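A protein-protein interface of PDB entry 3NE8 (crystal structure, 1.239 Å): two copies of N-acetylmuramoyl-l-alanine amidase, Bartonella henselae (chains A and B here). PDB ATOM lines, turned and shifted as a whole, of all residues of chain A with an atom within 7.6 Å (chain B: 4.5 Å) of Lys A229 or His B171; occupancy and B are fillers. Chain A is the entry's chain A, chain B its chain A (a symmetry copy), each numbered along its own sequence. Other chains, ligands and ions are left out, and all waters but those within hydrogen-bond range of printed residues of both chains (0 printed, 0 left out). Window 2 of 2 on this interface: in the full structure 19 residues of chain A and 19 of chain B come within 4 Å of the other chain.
The side-chain amino group of Lys A229 is in hydrogen-bond range of the side-chain amide oxygen of Asn B153 (3.1 Å).
A ring nitrogen (ND1) of His B171 is in hydrogen-bond range of the side-chain amino group of Lys A229 (3.0 Å).
N of Met A231 is in hydrogen-bond range of ND1 of His B145, at 2.9 Å.
The side-chain hydroxyl of Thr B98 sits at hydrogen-bond distance from a ring nitrogen (NE2) of His B171.
Among the printed residues, pairs that only touch across the chains: Tyr A226 with Ile B149, Tyr A226 with Asn B153, Lys A229 with His B145 and Ile A230 with His B145.
Printed residues of chain B within 4 Å of Lys A229: His B145, Asn B153 and His B171.
Of chain A, only Lys A229 (3.0 Å) comes within 4 Å of His B171.
Of the printed residues of chain A, His B145 touches Lys A229, Ile A230 and Met A231.
Of the printed residues of chain B, Tyr A226 touches Ile B149 and Asn B153.
Printed residues of chain B within 4 Å of Met A231: His B145.
Printed residues of chain A within 4 Å of Asn B153: Tyr A226 (3.9 Å) and Lys A229 (3.1 Å).
Of the printed residues of chain B, Ile A230 touches His B145.
Val B96 touches none of the printed residues of chain A.
Gln A232 touches none of the printed residues of chain B.
The nearest printed residue of chain B that does not touch Lys A229 is Ile B149 (4.03 Å).
The nearest printed residue of chain A that does not touch His B171 is Ile A230 (7.7 Å).
The nearest printed residue of chain A that does not touch Asn B153 is Glu A225 (6.5 Å).
Hydrophobic or aromatic side chains of chain B that line the printed part of chain A: His B145, Ile B149 and His B171.
Among the printed residues, 7 pairs touch across the chains.
No position is printed for both chains.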
ATOM      1  N   PHE A 223      31.382   4.001  29.044  1.00  0.00           N
ATOM      2  CA  PHE A 223      32.324   5.025  28.619  1.00  0.00           C
ATOM      3  C   PHE A 223      33.162   4.551  27.429  1.00  0.00           C
ATOM      4  O   PHE A 223      33.391   5.311  26.483  1.00  0.00           O
ATOM      5  CB  PHE A 223      33.201   5.390  29.815  1.00  0.00           C
ATOM      6  CG  PHE A 223      34.156   6.525  29.578  1.00  0.00           C
ATOM      7  CD1 PHE A 223      33.691   7.818  29.373  1.00  0.00           C
ATOM      8  CD2 PHE A 223      35.523   6.306  29.632  1.00  0.00           C
ATOM      9  CE1 PHE A 223      34.581   8.869  29.204  1.00  0.00           C
ATOM     10  CE2 PHE A 223      36.418   7.346  29.459  1.00  0.00           C
ATOM     11  CZ  PHE A 223      35.946   8.635  29.242  1.00  0.00           C
ATOM     12  N   ALA A 224      33.587   3.289  27.461  1.00  0.00           N
ATOM     13  CA  ALA A 224      34.341   2.712  26.353  1.00  0.00           C
ATOM     14  C   ALA A 224      33.505   2.722  25.075  1.00  0.00           C
ATOM     15  O   ALA A 224      33.994   3.066  23.995  1.00  0.00           O
ATOM     16  CB  ALA A 224      34.760   1.295  26.687  1.00  0.00           C
ATOM     17  N   GLU A 225      32.245   2.326  25.183  1.00  0.00           N
ATOM     18  CA  GLU A 225      31.396   2.277  24.002  1.00  0.00           C
ATOM     19  C   GLU A 225      31.222   3.666  23.402  1.00  0.00           C
ATOM     20  O   GLU A 225      31.237   3.822  22.177  1.00  0.00           O
ATOM     21  CB  GLU A 225      30.048   1.636  24.326  1.00  0.00           C
ATOM     22  CG  GLU A 225      30.153   0.147  24.620  1.00  0.00           C
ATOM     23  CD  GLU A 225      28.884  -0.440  25.213  1.00  0.00           C
ATOM     24  OE1 GLU A 225      27.929   0.323  25.464  1.00  0.00           O
ATOM     25  OE2 GLU A 225      28.849  -1.668  25.435  1.00  0.00           O
ATOM     26  N   TYR A 226      31.085   4.668  24.262  1.00  0.00           N
ATOM     27  CA  TYR A 226      30.987   6.055  23.838  1.00  0.00           C
ATOM     28  C   TYR A 226      32.270   6.514  23.152  1.00  0.00           C
ATOM     29  O   TYR A 226      32.233   7.036  22.029  1.00  0.00           O
ATOM     30  CB  TYR A 226      30.678   6.926  25.057  1.00  0.00           C
ATOM     31  CG  TYR A 226      30.939   8.400  24.861  1.00  0.00           C
ATOM     32  CD1 TYR A 226      30.281   9.116  23.876  1.00  0.00           C
ATOM     33  CD2 TYR A 226      31.818   9.086  25.673  1.00  0.00           C
ATOM     34  CE1 TYR A 226      30.514  10.474  23.690  1.00  0.00           C
ATOM     35  CE2 TYR A 226      32.051  10.433  25.498  1.00  0.00           C
ATOM     36  CZ  TYR A 226      31.401  11.120  24.504  1.00  0.00           C
ATOM     37  OH  TYR A 226      31.656  12.467  24.351  1.00  0.00           O
ATOM     38  N   ARG A 227      33.405   6.302  23.812  1.00  0.00           N
ATOM     39  CA  ARG A 227      34.699   6.732  23.287  1.00  0.00           C
ATOM     40  C   ARG A 227      34.962   6.147  21.904  1.00  0.00           C
ATOM     41  O   ARG A 227      35.526   6.809  21.029  1.00  0.00           O
ATOM     42  CB  ARG A 227      35.829   6.327  24.238  1.00  0.00           C
ATOM     43  CG  ARG A 227      35.803   7.035  25.578  1.00  0.00           C
ATOM     44  CD  ARG A 227      36.258   8.476  25.456  1.00  0.00           C
ATOM     45  NE  ARG A 227      37.582   8.592  24.846  1.00  0.00           N
ATOM     46  CZ  ARG A 227      38.728   8.434  25.498  1.00  0.00           C
ATOM     47  NH1 ARG A 227      38.727   8.136  26.794  1.00  0.00           N
ATOM     48  NH2 ARG A 227      39.878   8.564  24.853  1.00  0.00           N
ATOM     49  N   GLN A 228      34.552   4.904  21.701  1.00  0.00           N
ATOM     50  CA  GLN A 228      34.842   4.234  20.444  1.00  0.00           C
ATOM     51  C   GLN A 228      33.962   4.690  19.271  1.00  0.00           C
ATOM     52  O   GLN A 228      34.251   4.373  18.120  1.00  0.00           O
ATOM     53  CB  GLN A 228      34.836   2.715  20.646  1.00  0.00           C
ATOM     54  CG  GLN A 228      35.961   2.281  21.586  1.00  0.00           C
ATOM     55  CD  GLN A 228      35.885   0.831  22.016  1.00  0.00           C
ATOM     56  OE1 GLN A 228      36.819   0.309  22.623  1.00  0.00           O
ATOM     57  NE2 GLN A 228      34.774   0.174  21.710  1.00  0.00           N
ATOM     58  N   LYS A 229      32.916   5.463  19.560  1.00  0.00           N
ATOM     59  CA  LYS A 229      32.068   6.041  18.522  1.00  0.00           C
ATOM     60  C   LYS A 229      32.692   7.296  17.903  1.00  0.00           C
ATOM     61  O   LYS A 229      32.273   7.734  16.831  1.00  0.00           O
ATOM     62  CB  LYS A 229      30.699   6.419  19.093  1.00  0.00           C
ATOM     63  CG  LYS A 229      29.767   5.264  19.405  1.00  0.00           C
ATOM     64  CD  LYS A 229      28.427   5.817  19.875  1.00  0.00           C
ATOM     65  CE  LYS A 229      27.354   4.752  19.976  1.00  0.00           C
ATOM     66  NZ  LYS A 229      26.022   5.380  20.233  1.00  0.00           N
ATOM     67  N   ILE A 230      33.683   7.870  18.575  1.00  0.00           N
ATOM     68  CA  ILE A 230      34.216   9.182  18.194  1.00  0.00           C
ATOM     69  C   ILE A 230      35.254   9.085  17.077  1.00  0.00           C
ATOM     70  O   ILE A 230      36.065   8.155  17.052  1.00  0.00           O
ATOM     71  CB  ILE A 230      34.762   9.921  19.434  1.00  0.00           C
ATOM     72  CG1 ILE A 230      33.654   9.995  20.491  1.00  0.00           C
ATOM     73  CG2 ILE A 230      35.277  11.308  19.066  1.00  0.00           C
ATOM     74  CD1 ILE A 230      34.101  10.484  21.840  1.00  0.00           C
ATOM     75  N   MET A 231      35.228  10.039  16.156  1.00  0.00           N
ATOM     76  CA  MET A 231      36.078   9.982  14.972  1.00  0.00           C
ATOM     77  C   MET A 231      37.557  10.134  15.298  1.00  0.00           C
ATOM     78  O   MET A 231      37.934  10.679  16.336  1.00  0.00           O
ATOM     79  CB  MET A 231      35.689  11.088  13.996  1.00  0.00           C
ATOM     80  CG  MET A 231      35.983  12.491  14.515  1.00  0.00           C
ATOM     81  SD  MET A 231      35.787  13.880  13.168  1.00  0.00           S
ATOM     82  CE  MET A 231      33.960  13.480  12.616  1.00  0.00           C
ATOM     83  N   GLN A 232      38.391   9.629  14.393  1.00  0.00           N
ATOM     84  CA  GLN A 232      39.825   9.879  14.451  1.00  0.00           C
ATOM     85  C   GLN A 232      40.239  10.554  13.153  1.00  0.00           C
ATOM     86  O   GLN A 232      40.463   9.902  12.129  1.00  0.00           O
ATOM     87  CB  GLN A 232      40.629   8.599  14.683  1.00  0.00           C
ATOM     88  CG  GLN A 232      41.662   8.727  15.807  1.00  0.00           C
ATOM     89  CD  GLN A 232      42.439  10.039  15.758  1.00  0.00           C
ATOM     90  OE1 GLN A 232      42.641  10.700  16.785  1.00  0.00           O
ATOM     91  NE2 GLN A 232      42.877  10.421  14.561  1.00  0.00           N
ATOM     92  N   VAL B  96      18.400   9.799  15.406  1.00  0.00           N
ATOM     93  CA  VAL B  96      19.398  10.863  15.479  1.00  0.00           C
ATOM     94  C   VAL B  96      20.630  10.447  14.694  1.00  0.00           C
ATOM     95  O   VAL B  96      21.168   9.343  14.895  1.00  0.00           O
ATOM     96  CB  VAL B  96      19.801  11.206  16.924  1.00  0.00           C
ATOM     97  CG1 VAL B  96      20.712  12.431  16.933  1.00  0.00           C
ATOM     98  CG2 VAL B  96      18.579  11.446  17.787  1.00  0.00           C
ATOM     99  N   THR B  98      24.601  11.529  13.444  1.00  0.00           N
ATOM    100  CA  THR B  98      25.809  12.342  13.536  1.00  0.00           C
ATOM    101  C   THR B  98      26.628  12.147  12.264  1.00  0.00           C
ATOM    102  O   THR B  98      26.323  11.255  11.461  1.00  0.00           O
ATOM    103  CB  THR B  98      26.643  11.968  14.771  1.00  0.00           C
ATOM    104  OG1 THR B  98      26.790  10.543  14.846  1.00  0.00           O
ATOM    105  CG2 THR B  98      25.937  12.445  16.019  1.00  0.00           C
ATOM    106  N   HIS B 145      33.122  16.403  17.658  1.00  0.00           N
ATOM    107  CA  HIS B 145      32.447  15.145  17.408  1.00  0.00           C
ATOM    108  C   HIS B 145      32.070  14.435  18.711  1.00  0.00           C
ATOM    109  O   HIS B 145      30.995  13.853  18.826  1.00  0.00           O
ATOM    110  CB  HIS B 145      33.310  14.250  16.527  1.00  0.00           C
ATOM    111  CG  HIS B 145      32.546  13.131  15.909  1.00  0.00           C
ATOM    112  ND1 HIS B 145      32.926  11.814  16.022  1.00  0.00           N
ATOM    113  CD2 HIS B 145      31.404  13.137  15.182  1.00  0.00           C
ATOM    114  CE1 HIS B 145      32.054  11.054  15.383  1.00  0.00           C
ATOM    115  NE2 HIS B 145      31.120  11.831  14.867  1.00  0.00           N
ATOM    116  N   ILE B 149      28.189  13.310  19.533  1.00  0.00           N
ATOM    117  CA  ILE B 149      27.876  11.942  19.953  1.00  0.00           C
ATOM    118  C   ILE B 149      27.174  11.941  21.315  1.00  0.00           C
ATOM    119  O   ILE B 149      26.176  11.250  21.532  1.00  0.00           O
ATOM    120  CB  ILE B 149      29.176  11.077  20.040  1.00  0.00           C
ATOM    121  CG1 ILE B 149      29.804  10.852  18.655  1.00  0.00           C
ATOM    122  CG2 ILE B 149      28.898   9.734  20.701  1.00  0.00           C
ATOM    123  CD1 ILE B 149      28.930  10.074  17.693  1.00  0.00           C
ATOM    124  N   ALA B 152      23.651  13.226  20.881  1.00  0.00           N
ATOM    125  CA  ALA B 152      22.830  12.213  20.222  1.00  0.00           C
ATOM    126  C   ALA B 152      22.405  11.125  21.213  1.00  0.00           C
ATOM    127  O   ALA B 152      21.238  10.716  21.252  1.00  0.00           O
ATOM    128  CB  ALA B 152      23.574  11.596  19.028  1.00  0.00           C
ATOM    129  N   ASN B 153      23.367  10.646  22.005  1.00  0.00           N
ATOM    130  CA  ASN B 153      23.105   9.601  22.996  1.00  0.00           C
ATOM    131  C   ASN B 153      22.070  10.030  24.001  1.00  0.00           C
ATOM    132  O   ASN B 153      21.160   9.264  24.343  1.00  0.00           O
ATOM    133  CB  ASN B 153      24.382   9.252  23.765  1.00  0.00           C
ATOM    134  CG  ASN B 153      25.274   8.303  23.014  1.00  0.00           C
ATOM    135  OD1 ASN B 153      24.849   7.660  22.052  1.00  0.00           O
ATOM    136  ND2 ASN B 153      26.528   8.198  23.453  1.00  0.00           N
ATOM    137  N   VAL B 156      18.451  10.211  22.456  1.00  0.00           N
ATOM    138  CA  VAL B 156      17.878   8.877  22.354  1.00  0.00           C
ATOM    139  C   VAL B 156      17.424   8.365  23.721  1.00  0.00           C
ATOM    140  O   VAL B 156      16.315   7.861  23.859  1.00  0.00           O
ATOM    141  CB  VAL B 156      18.888   7.895  21.735  1.00  0.00           C
ATOM    142  CG1 VAL B 156      18.447   6.453  21.968  1.00  0.00           C
ATOM    143  CG2 VAL B 156      19.079   8.196  20.254  1.00  0.00           C
ATOM    144  N   ASN B 169      18.139   0.755  16.299  1.00  0.00           N
ATOM    145  CA  ASN B 169      19.431   1.433  16.160  1.00  0.00           C
ATOM    146  C   ASN B 169      19.232   2.930  15.924  1.00  0.00           C
ATOM    147  O   ASN B 169      19.528   3.439  14.840  1.00  0.00           O
ATOM    148  CB  ASN B 169      20.239   0.835  15.003  1.00  0.00           C
ATOM    149  CG  ASN B 169      20.628  -0.605  15.244  1.00  0.00           C
ATOM    150  OD1 ASN B 169      20.724  -1.398  14.309  1.00  0.00           O
ATOM    151  ND2 ASN B 169      20.853  -0.952  16.501  1.00  0.00           N
ATOM    152  N   PRO B 170      18.714   3.638  16.935  1.00  0.00           N
ATOM    153  CA  PRO B 170      18.261   5.018  16.717  1.00  0.00           C
ATOM    154  C   PRO B 170      19.378   6.056  16.637  1.00  0.00           C
ATOM    155  O   PRO B 170      19.079   7.194  16.266  1.00  0.00           O
ATOM    156  CB  PRO B 170      17.366   5.280  17.931  1.00  0.00           C
ATOM    157  CG  PRO B 170      17.959   4.439  19.000  1.00  0.00           C
ATOM    158  CD  PRO B 170      18.432   3.176  18.306  1.00  0.00           C
ATOM    159  N   HIS B 171      20.613   5.703  16.978  1.00  0.00           N
ATOM    160  CA  HIS B 171      21.737   6.579  16.676  1.00  0.00           C
ATOM    161  C   HIS B 171      22.488   6.038  15.470  1.00  0.00           C
ATOM    162  O   HIS B 171      23.122   4.988  15.555  1.00  0.00           O
ATOM    163  CB  HIS B 171      22.691   6.751  17.862  1.00  0.00           C
ATOM    164  CG  HIS B 171      23.917   7.536  17.517  1.00  0.00           C
ATOM    165  ND1 HIS B 171      25.175   7.212  17.978  1.00  0.00           N
ATOM    166  CD2 HIS B 171      24.082   8.599  16.697  1.00  0.00           C
ATOM    167  CE1 HIS B 171      26.055   8.066  17.485  1.00  0.00           C
ATOM    168  NE2 HIS B 171      25.415   8.919  16.704  1.00  0.00           N
ATOM    169  N   ARG B 172      22.398   6.753  14.354  1.00  0.00           N
ATOM    170  CA  ARG B 172      23.050   6.366  13.113  1.00  0.00           C
ATOM    171  C   ARG B 172      23.981   7.477  12.648  1.00  0.00           C
ATOM    172  O   ARG B 172      24.100   8.522  13.295  1.00  0.00           O
ATOM    173  CB  ARG B 172      22.006   6.019  12.049  1.00  0.00           C
ATOM    174  CG  ARG B 172      21.092   4.890  12.492  1.00  0.00           C
ATOM    175  CD  ARG B 172      20.140   4.425  11.415  1.00  0.00           C
ATOM    176  NE  ARG B 172      19.250   3.388  11.936  1.00  0.00           N
ATOM    177  CZ  ARG B 172      18.654   2.463  11.193  1.00  0.00           C
ATOM    178  NH1 ARG B 172      18.850   2.426   9.881  1.00  0.00           N
ATOM    179  NH2 ARG B 172      17.860   1.572  11.772  1.00  0.00           N
